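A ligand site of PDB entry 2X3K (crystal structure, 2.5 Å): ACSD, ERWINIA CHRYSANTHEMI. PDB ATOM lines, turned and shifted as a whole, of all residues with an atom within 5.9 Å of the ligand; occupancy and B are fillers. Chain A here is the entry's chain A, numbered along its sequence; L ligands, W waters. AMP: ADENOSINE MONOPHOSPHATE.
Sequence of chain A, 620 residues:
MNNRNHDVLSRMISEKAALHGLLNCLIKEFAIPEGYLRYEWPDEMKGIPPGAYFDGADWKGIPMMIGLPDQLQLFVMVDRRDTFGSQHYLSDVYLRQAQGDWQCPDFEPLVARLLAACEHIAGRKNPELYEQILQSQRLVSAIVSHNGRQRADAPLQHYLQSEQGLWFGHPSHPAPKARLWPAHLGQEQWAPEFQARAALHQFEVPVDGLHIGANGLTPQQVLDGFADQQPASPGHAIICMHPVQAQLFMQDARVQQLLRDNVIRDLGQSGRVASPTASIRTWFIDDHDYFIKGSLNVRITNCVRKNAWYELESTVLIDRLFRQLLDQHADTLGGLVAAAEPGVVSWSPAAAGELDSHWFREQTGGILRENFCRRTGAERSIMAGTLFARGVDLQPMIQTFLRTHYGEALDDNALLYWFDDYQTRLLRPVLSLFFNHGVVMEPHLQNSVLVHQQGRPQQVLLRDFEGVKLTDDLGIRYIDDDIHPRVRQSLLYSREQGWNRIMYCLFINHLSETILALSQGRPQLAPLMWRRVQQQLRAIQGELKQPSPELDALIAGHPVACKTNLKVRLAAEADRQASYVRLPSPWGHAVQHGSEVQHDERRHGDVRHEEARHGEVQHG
The side-chain hydroxyl (OG1) of Thr 301 is in hydrogen-bond range of an oxygen (O2') of the ligand.
An oxygen (O3P) of the ligand lies within salt-bridge range of the guanidinium group of Arg 305, at 2.8 Å.
A nitrogen (N7) of the ligand lies close to the backbone NH (N) of His 170 (3.4 Å).
The side-chain amide oxygen (OE1) of Gln 446 sits close to an oxygen (O1P) of the ligand (3.4 Å).
A nitrogen (N1) of the ligand is in hydrogen-bond range of the side-chain amide nitrogen (ND2) of Asn 509 (3.1 Å).
The backbone carbonyl oxygen (O) of Leu 445 lies within hydrogen-bond range of the backbone NH (N) of Gly 385 (3.0 Å).
OD1 of Asn 509 lies within hydrogen-bond range of N of Leu 445.
N of Asn 509 is in hydrogen-bond range of O of Tyr 504 (2.9 Å).
NH2 of Arg 305 lies within hydrogen-bond range of O of Ile 300, 2.6 Å away.
The backbone NH (N) of Gln 446 sits at hydrogen-bond distance from a ring nitrogen (ND1) of His 444 (3.2 Å).
The side-chain amide oxygen (OD1) of Asn 447 lies close to the side-chain carboxylate (OD2) of Asp 464, 3.4 Å away.
The side-chain amide oxygen of Gln 446 sits close to the side-chain amide oxygen of Asn 447.
The side-chain carboxylate of Asp 464 lies close to the backbone NH of Glu 466 (3.4 Å).
Water W1 lies within hydrogen-bond range of O of Pro 176 (2.8 Å), N of His 170 (2.9 Å) and O2' of the ligand (3.1 Å).
Water W2 bridges O of Asn 509 (2.9 Å) and N6 of the ligand (3.3 Å).
An oxygen (O1P) of the ligand lies close to the side-chain carboxylate (OD2) of Asp 464, 3.3 Å away.
Merely in contact with the ligand: Leu 166 (3.7 Å), Gly 169 (3.996 Å), Pro 171 (3.97 Å), Ile 300 (3.99 Å), His 444 (3.2 Å) and Leu 445 (3.7 Å).
12 residues have an atom within 4 Å of the ligand: Leu 166, Gly 169, His 170, Pro 171, Ile 300, Thr 301, Arg 305, His 444, Leu 445, Gln 446, Asp 464 and Asn 509.
Along chain A the residues within 4 Å of the ligand span positions 166 to 509.
The nearest printed residue that does not touch the ligand is Asn 447 (4.1 Å).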
ATOM      1  N   LEU A 166      34.833 -16.330   1.825  1.00  0.00           N
ATOM      2  CA  LEU A 166      33.530 -16.989   1.943  1.00  0.00           C
ATOM      3  C   LEU A 166      33.737 -18.467   2.418  1.00  0.00           C
ATOM      4  O   LEU A 166      33.459 -19.479   1.679  1.00  0.00           O
ATOM      5  CB  LEU A 166      32.730 -16.924   0.651  1.00  0.00           C
ATOM      6  CG  LEU A 166      31.223 -17.214   0.775  1.00  0.00           C
ATOM      7  CD1 LEU A 166      30.542 -16.136   1.617  1.00  0.00           C
ATOM      8  CD2 LEU A 166      30.580 -17.298  -0.600  1.00  0.00           C
ATOM      9  N   GLY A 169      30.558 -20.651   1.996  1.00  0.00           N
ATOM     10  CA  GLY A 169      29.850 -20.628   0.716  1.00  0.00           C
ATOM     11  C   GLY A 169      28.416 -20.181   0.872  1.00  0.00           C
ATOM     12  O   GLY A 169      28.092 -19.466   1.832  1.00  0.00           O
ATOM     13  N   HIS A 170      27.553 -20.608  -0.058  1.00  0.00           N
ATOM     14  CA  HIS A 170      26.087 -20.401   0.034  1.00  0.00           C
ATOM     15  C   HIS A 170      25.500 -20.996   1.353  1.00  0.00           C
ATOM     16  O   HIS A 170      25.493 -22.204   1.554  1.00  0.00           O
ATOM     17  CB  HIS A 170      25.456 -21.020  -1.205  1.00  0.00           C
ATOM     18  CG  HIS A 170      24.025 -20.652  -1.453  1.00  0.00           C
ATOM     19  ND1 HIS A 170      23.085 -20.516  -0.442  1.00  0.00           N
ATOM     20  CD2 HIS A 170      23.357 -20.487  -2.616  1.00  0.00           C
ATOM     21  CE1 HIS A 170      21.912 -20.251  -0.977  1.00  0.00           C
ATOM     22  NE2 HIS A 170      22.046 -20.209  -2.288  1.00  0.00           N
ATOM     23  N   PRO A 171      24.994 -20.139   2.240  1.00  0.00           N
ATOM     24  CA  PRO A 171      24.527 -20.585   3.542  1.00  0.00           C
ATOM     25  C   PRO A 171      23.196 -21.360   3.535  1.00  0.00           C
ATOM     26  O   PRO A 171      22.740 -21.779   4.606  1.00  0.00           O
ATOM     27  CB  PRO A 171      24.315 -19.253   4.304  1.00  0.00           C
ATOM     28  CG  PRO A 171      23.922 -18.314   3.225  1.00  0.00           C
ATOM     29  CD  PRO A 171      24.813 -18.671   2.081  1.00  0.00           C
ATOM     30  N   HIS A 173      22.360 -24.204   1.310  1.00  0.00           N
ATOM     31  CA  HIS A 173      22.740 -25.142   0.272  1.00  0.00           C
ATOM     32  C   HIS A 173      23.314 -26.345   0.991  1.00  0.00           C
ATOM     33  O   HIS A 173      23.966 -26.195   2.025  1.00  0.00           O
ATOM     34  CB  HIS A 173      23.792 -24.508  -0.613  1.00  0.00           C
ATOM     35  CG  HIS A 173      24.046 -25.245  -1.878  1.00  0.00           C
ATOM     36  ND1 HIS A 173      24.704 -26.461  -1.913  1.00  0.00           N
ATOM     37  CD2 HIS A 173      23.749 -24.945  -3.164  1.00  0.00           C
ATOM     38  CE1 HIS A 173      24.772 -26.886  -3.162  1.00  0.00           C
ATOM     39  NE2 HIS A 173      24.190 -25.990  -3.940  1.00  0.00           N
ATOM     40  N   PRO A 176      27.825 -26.528  -0.272  1.00  0.00           N
ATOM     41  CA  PRO A 176      28.305 -25.244  -0.801  1.00  0.00           C
ATOM     42  C   PRO A 176      29.702 -25.258  -1.398  1.00  0.00           C
ATOM     43  O   PRO A 176      29.994 -24.447  -2.273  1.00  0.00           O
ATOM     44  CB  PRO A 176      28.274 -24.321   0.426  1.00  0.00           C
ATOM     45  CG  PRO A 176      28.231 -25.259   1.616  1.00  0.00           C
ATOM     46  CD  PRO A 176      27.442 -26.418   1.145  1.00  0.00           C
ATOM     47  N   ALA A 278      35.273 -16.075  -5.721  1.00  0.00           N
ATOM     48  CA  ALA A 278      34.295 -17.023  -5.174  1.00  0.00           C
ATOM     49  C   ALA A 278      33.530 -17.899  -6.160  1.00  0.00           C
ATOM     50  O   ALA A 278      33.144 -19.033  -5.815  1.00  0.00           O
ATOM     51  CB  ALA A 278      33.301 -16.318  -4.222  1.00  0.00           C
ATOM     52  N   SER A 279      33.275 -17.397  -7.376  1.00  0.00           N
ATOM     53  CA  SER A 279      32.655 -18.212  -8.414  1.00  0.00           C
ATOM     54  C   SER A 279      33.633 -19.164  -9.086  1.00  0.00           C
ATOM     55  O   SER A 279      33.239 -19.802 -10.065  1.00  0.00           O
ATOM     56  CB  SER A 279      32.115 -17.325  -9.494  1.00  0.00           C
ATOM     57  OG  SER A 279      33.218 -16.767 -10.144  1.00  0.00           O
ATOM     58  N   ILE A 280      34.901 -19.191  -8.668  1.00  0.00           N
ATOM     59  CA  ILE A 280      35.907 -20.196  -9.114  1.00  0.00           C
ATOM     60  C   ILE A 280      36.428 -20.060 -10.561  1.00  0.00           C
ATOM     61  O   ILE A 280      37.648 -20.106 -10.833  1.00  0.00           O
ATOM     62  CB  ILE A 280      35.376 -21.678  -8.933  1.00  0.00           C
ATOM     63  CG1 ILE A 280      34.837 -21.875  -7.508  1.00  0.00           C
ATOM     64  CG2 ILE A 280      36.428 -22.683  -9.333  1.00  0.00           C
ATOM     65  CD1 ILE A 280      35.806 -21.524  -6.367  1.00  0.00           C
ATOM     66  N   ARG A 281      35.505 -19.932 -11.498  1.00  0.00           N
ATOM     67  CA  ARG A 281      35.911 -19.704 -12.895  1.00  0.00           C
ATOM     68  C   ARG A 281      36.193 -18.222 -13.295  1.00  0.00           C
ATOM     69  O   ARG A 281      36.436 -17.932 -14.488  1.00  0.00           O
ATOM     70  CB  ARG A 281      34.897 -20.352 -13.845  1.00  0.00           C
ATOM     71  CG  ARG A 281      33.451 -20.049 -13.554  1.00  0.00           C
ATOM     72  CD  ARG A 281      32.935 -18.775 -14.249  1.00  0.00           C
ATOM     73  NE  ARG A 281      31.474 -18.825 -14.406  1.00  0.00           N
ATOM     74  CZ  ARG A 281      30.819 -18.959 -15.548  1.00  0.00           C
ATOM     75  NH1 ARG A 281      31.417 -19.024 -16.720  1.00  0.00           N
ATOM     76  NH2 ARG A 281      29.506 -19.010 -15.509  1.00  0.00           N
ATOM     77  N   ILE A 300      30.154 -27.297 -10.308  1.00  0.00           N
ATOM     78  CA  ILE A 300      30.388 -26.599  -9.048  1.00  0.00           C
ATOM     79  C   ILE A 300      29.031 -26.191  -8.525  1.00  0.00           C
ATOM     80  O   ILE A 300      28.311 -25.439  -9.187  1.00  0.00           O
ATOM     81  CB  ILE A 300      31.293 -25.323  -9.204  1.00  0.00           C
ATOM     82  CG1 ILE A 300      32.784 -25.650  -9.003  1.00  0.00           C
ATOM     83  CG2 ILE A 300      30.998 -24.278  -8.137  1.00  0.00           C
ATOM     84  CD1 ILE A 300      33.344 -26.714  -9.907  1.00  0.00           C
ATOM     85  N   THR A 301      28.688 -26.680  -7.326  1.00  0.00           N
ATOM     86  CA  THR A 301      27.383 -26.457  -6.728  1.00  0.00           C
ATOM     87  C   THR A 301      26.351 -27.107  -7.652  1.00  0.00           C
ATOM     88  O   THR A 301      26.540 -28.258  -8.110  1.00  0.00           O
ATOM     89  CB  THR A 301      27.091 -24.929  -6.570  1.00  0.00           C
ATOM     90  OG1 THR A 301      28.215 -24.259  -5.977  1.00  0.00           O
ATOM     91  CG2 THR A 301      25.866 -24.679  -5.716  1.00  0.00           C
ATOM     92  N   CYS A 303      25.207 -26.364 -10.818  1.00  0.00           N
ATOM     93  CA  CYS A 303      25.294 -26.212 -12.281  1.00  0.00           C
ATOM     94  C   CYS A 303      26.693 -26.462 -12.899  1.00  0.00           C
ATOM     95  O   CYS A 303      27.725 -26.584 -12.202  1.00  0.00           O
ATOM     96  CB  CYS A 303      24.795 -24.811 -12.697  1.00  0.00           C
ATOM     97  SG  CYS A 303      23.412 -24.148 -11.668  1.00  0.00           S
ATOM     98  N   ARG A 305      29.526 -24.772 -15.102  1.00  0.00           N
ATOM     99  CA  ARG A 305      29.904 -23.371 -15.336  1.00  0.00           C
ATOM    100  C   ARG A 305      30.570 -23.123 -16.682  1.00  0.00           C
ATOM    101  O   ARG A 305      31.736 -22.756 -16.766  1.00  0.00           O
ATOM    102  CB  ARG A 305      30.729 -22.823 -14.175  1.00  0.00           C
ATOM    103  CG  ARG A 305      30.299 -23.346 -12.801  1.00  0.00           C
ATOM    104  CD  ARG A 305      29.044 -22.636 -12.336  1.00  0.00           C
ATOM    105  NE  ARG A 305      28.418 -23.190 -11.139  1.00  0.00           N
ATOM    106  CZ  ARG A 305      27.305 -22.698 -10.597  1.00  0.00           C
ATOM    107  NH1 ARG A 305      26.692 -21.647 -11.114  1.00  0.00           N
ATOM    108  NH2 ARG A 305      26.806 -23.288  -9.525  1.00  0.00           N
ATOM    109  N   GLY A 385      28.048 -11.485  -0.071  1.00  0.00           N
ATOM    110  CA  GLY A 385      28.048 -12.829   0.482  1.00  0.00           C
ATOM    111  C   GLY A 385      28.868 -12.929   1.732  1.00  0.00           C
ATOM    112  O   GLY A 385      28.379 -13.367   2.751  1.00  0.00           O
ATOM    113  N   GLU A 442      19.881 -10.622 -11.514  1.00  0.00           N
ATOM    114  CA  GLU A 442      19.946 -11.715 -10.561  1.00  0.00           C
ATOM    115  C   GLU A 442      20.694 -11.315  -9.285  1.00  0.00           C
ATOM    116  O   GLU A 442      21.722 -11.912  -8.947  1.00  0.00           O
ATOM    117  CB  GLU A 442      20.507 -12.988 -11.203  1.00  0.00           C
ATOM    118  CG  GLU A 442      20.532 -14.135 -10.204  1.00  0.00           C
ATOM    119  CD  GLU A 442      20.743 -15.549 -10.790  1.00  0.00           C
ATOM    120  OE1 GLU A 442      21.444 -15.719 -11.812  1.00  0.00           O
ATOM    121  OE2 GLU A 442      20.190 -16.496 -10.189  1.00  0.00           O
ATOM    122  N   HIS A 444      21.345 -11.818  -6.175  1.00  0.00           N
ATOM    123  CA  HIS A 444      21.729 -12.601  -4.965  1.00  0.00           C
ATOM    124  C   HIS A 444      23.060 -12.102  -4.416  1.00  0.00           C
ATOM    125  O   HIS A 444      23.761 -11.323  -5.069  1.00  0.00           O
ATOM    126  CB  HIS A 444      21.770 -14.151  -5.204  1.00  0.00           C
ATOM    127  CG  HIS A 444      22.720 -14.585  -6.269  1.00  0.00           C
ATOM    128  ND1 HIS A 444      24.087 -14.403  -6.175  1.00  0.00           N
ATOM    129  CD2 HIS A 444      22.508 -15.186  -7.467  1.00  0.00           C
ATOM    130  CE1 HIS A 444      24.671 -14.839  -7.286  1.00  0.00           C
ATOM    131  NE2 HIS A 444      23.732 -15.319  -8.089  1.00  0.00           N
ATOM    132  N   LEU A 445      23.423 -12.576  -3.220  1.00  0.00           N
ATOM    133  CA  LEU A 445      24.637 -12.161  -2.500  1.00  0.00           C
ATOM    134  C   LEU A 445      25.992 -12.140  -3.231  1.00  0.00           C
ATOM    135  O   LEU A 445      26.889 -11.381  -2.826  1.00  0.00           O
ATOM    136  CB  LEU A 445      24.769 -13.025  -1.239  1.00  0.00           C
ATOM    137  CG  LEU A 445      23.711 -12.715  -0.166  1.00  0.00           C
ATOM    138  CD1 LEU A 445      23.996 -13.586   1.030  1.00  0.00           C
ATOM    139  CD2 LEU A 445      23.683 -11.162   0.234  1.00  0.00           C
ATOM    140  N   GLN A 446      26.174 -12.968  -4.258  1.00  0.00           N
ATOM    141  CA  GLN A 446      27.482 -13.037  -4.933  1.00  0.00           C
ATOM    142  C   GLN A 446      27.480 -12.145  -6.165  1.00  0.00           C
ATOM    143  O   GLN A 446      28.537 -11.795  -6.684  1.00  0.00           O
ATOM    144  CB  GLN A 446      27.889 -14.495  -5.271  1.00  0.00           C
ATOM    145  CG  GLN A 446      29.212 -14.663  -6.048  1.00  0.00           C
ATOM    146  CD  GLN A 446      29.005 -14.837  -7.567  1.00  0.00           C
ATOM    147  OE1 GLN A 446      27.883 -14.985  -8.059  1.00  0.00           O
ATOM    148  NE2 GLN A 446      30.090 -14.848  -8.288  1.00  0.00           N
ATOM    149  N   ASN A 447      26.299 -11.790  -6.647  1.00  0.00           N
ATOM    150  CA  ASN A 447      26.215 -10.816  -7.754  1.00  0.00           C
ATOM    151  C   ASN A 447      26.173  -9.399  -7.272  1.00  0.00           C
ATOM    152  O   ASN A 447      25.823  -8.519  -8.036  1.00  0.00           O
ATOM    153  CB  ASN A 447      25.018 -11.094  -8.649  1.00  0.00           C
ATOM    154  CG  ASN A 447      25.197 -12.320  -9.516  1.00  0.00           C
ATOM    155  OD1 ASN A 447      26.314 -12.741  -9.788  1.00  0.00           O
ATOM    156  ND2 ASN A 447      24.108 -12.876 -10.002  1.00  0.00           N
ATOM    157  N   ASP A 464      27.100  -9.487 -13.308  1.00  0.00           N
ATOM    158  CA  ASP A 464      26.867 -10.793 -13.932  1.00  0.00           C
ATOM    159  C   ASP A 464      25.730 -10.787 -14.917  1.00  0.00           C
ATOM    160  O   ASP A 464      24.557 -10.873 -14.533  1.00  0.00           O
ATOM    161  CB  ASP A 464      26.693 -11.920 -12.906  1.00  0.00           C
ATOM    162  CG  ASP A 464      26.782 -13.312 -13.523  1.00  0.00           C
ATOM    163  OD1 ASP A 464      27.132 -13.452 -14.715  1.00  0.00           O
ATOM    164  OD2 ASP A 464      26.500 -14.273 -12.800  1.00  0.00           O
ATOM    165  N   GLU A 466      25.424 -12.950 -17.654  1.00  0.00           N
ATOM    166  CA  GLU A 466      24.992 -14.296 -17.906  1.00  0.00           C
ATOM    167  C   GLU A 466      23.538 -14.514 -17.476  1.00  0.00           C
ATOM    168  O   GLU A 466      22.707 -14.885 -18.296  1.00  0.00           O
ATOM    169  CB  GLU A 466      25.937 -15.254 -17.194  1.00  0.00           C
ATOM    170  CG  GLU A 466      25.512 -16.736 -17.137  1.00  0.00           C
ATOM    171  CD  GLU A 466      26.693 -17.643 -16.785  1.00  0.00           C
ATOM    172  OE1 GLU A 466      27.522 -17.220 -15.939  1.00  0.00           O
ATOM    173  OE2 GLU A 466      26.808 -18.756 -17.355  1.00  0.00           O
ATOM    174  N   TYR A 504      12.897 -13.997  -5.144  1.00  0.00           N
ATOM    175  CA  TYR A 504      13.801 -14.907  -4.429  1.00  0.00           C
ATOM    176  C   TYR A 504      15.118 -14.218  -4.102  1.00  0.00           C
ATOM    177  O   TYR A 504      15.551 -14.263  -2.942  1.00  0.00           O
ATOM    178  CB  TYR A 504      14.079 -16.214  -5.181  1.00  0.00           C
ATOM    179  CG  TYR A 504      15.303 -16.935  -4.642  1.00  0.00           C
ATOM    180  CD1 TYR A 504      15.249 -17.627  -3.415  1.00  0.00           C
ATOM    181  CD2 TYR A 504      16.518 -16.896  -5.336  1.00  0.00           C
ATOM    182  CE1 TYR A 504      16.376 -18.276  -2.893  1.00  0.00           C
ATOM    183  CE2 TYR A 504      17.653 -17.525  -4.844  1.00  0.00           C
ATOM    184  CZ  TYR A 504      17.591 -18.221  -3.619  1.00  0.00           C
ATOM    185  OH  TYR A 504      18.738 -18.847  -3.135  1.00  0.00           O
ATOM    186  N   ASN A 509      17.145 -14.868  -0.581  1.00  0.00           N
ATOM    187  CA  ASN A 509      18.588 -14.950  -0.682  1.00  0.00           C
ATOM    188  C   ASN A 509      19.307 -13.794   0.009  1.00  0.00           C
ATOM    189  O   ASN A 509      20.310 -14.025   0.654  1.00  0.00           O
ATOM    190  CB  ASN A 509      19.025 -15.039  -2.168  1.00  0.00           C
ATOM    191  CG  ASN A 509      20.489 -15.429  -2.340  1.00  0.00           C
ATOM    192  OD1 ASN A 509      21.362 -14.557  -2.344  1.00  0.00           O
ATOM    193  ND2 ASN A 509      20.772 -16.763  -2.487  1.00  0.00           N
HETATM  194  P   AMP L   1      25.935 -18.151 -10.535  1.00  0.00           P
HETATM  195  O1P AMP L   1      26.479 -16.726 -10.601  1.00  0.00           O
HETATM  196  O2P AMP L   1      24.497 -18.249 -10.026  1.00  0.00           O
HETATM  197  O3P AMP L   1      26.243 -19.007 -11.741  1.00  0.00           O
HETATM  198  O5' AMP L   1      26.867 -18.725  -9.334  1.00  0.00           O
HETATM  199  C5' AMP L   1      27.495 -17.868  -8.371  1.00  0.00           C
HETATM  200  C4' AMP L   1      28.416 -18.599  -7.402  1.00  0.00           C
HETATM  201  O4' AMP L   1      28.363 -17.980  -6.101  1.00  0.00           O
HETATM  202  C3' AMP L   1      27.996 -20.055  -7.208  1.00  0.00           C
HETATM  203  O3' AMP L   1      29.166 -20.823  -7.368  1.00  0.00           O
HETATM  204  C2' AMP L   1      27.494 -20.152  -5.779  1.00  0.00           C
HETATM  205  O2' AMP L   1      27.764 -21.406  -5.145  1.00  0.00           O
HETATM  206  C1' AMP L   1      28.216 -19.019  -5.096  1.00  0.00           C
HETATM  207  N9  AMP L   1      27.391 -18.490  -3.998  1.00  0.00           N
HETATM  208  C8  AMP L   1      27.817 -18.386  -2.738  1.00  0.00           C
HETATM  209  N7  AMP L   1      26.846 -17.856  -1.973  1.00  0.00           N
HETATM  210  C5  AMP L   1      25.784 -17.615  -2.733  1.00  0.00           C
HETATM  211  C6  AMP L   1      24.459 -17.038  -2.511  1.00  0.00           C
HETATM  212  N6  AMP L   1      24.101 -16.646  -1.260  1.00  0.00           N
HETATM  213  N1  AMP L   1      23.640 -16.939  -3.591  1.00  0.00           N
HETATM  214  C2  AMP L   1      23.990 -17.329  -4.815  1.00  0.00           C
HETATM  215  N3  AMP L   1      25.211 -17.832  -5.077  1.00  0.00           N
HETATM  216  C4  AMP L   1      26.140 -18.013  -4.091  1.00  0.00           C
HETATM  217  O   HOH W   1      28.998 -21.813  -2.328  1.00  0.00           O
HETATM  218  O   HOH W   2      21.270 -16.720   0.408  1.00  0.00           O
HETATM  219  O   HOH W   3      26.525 -16.088   0.160  1.00  0.00           O
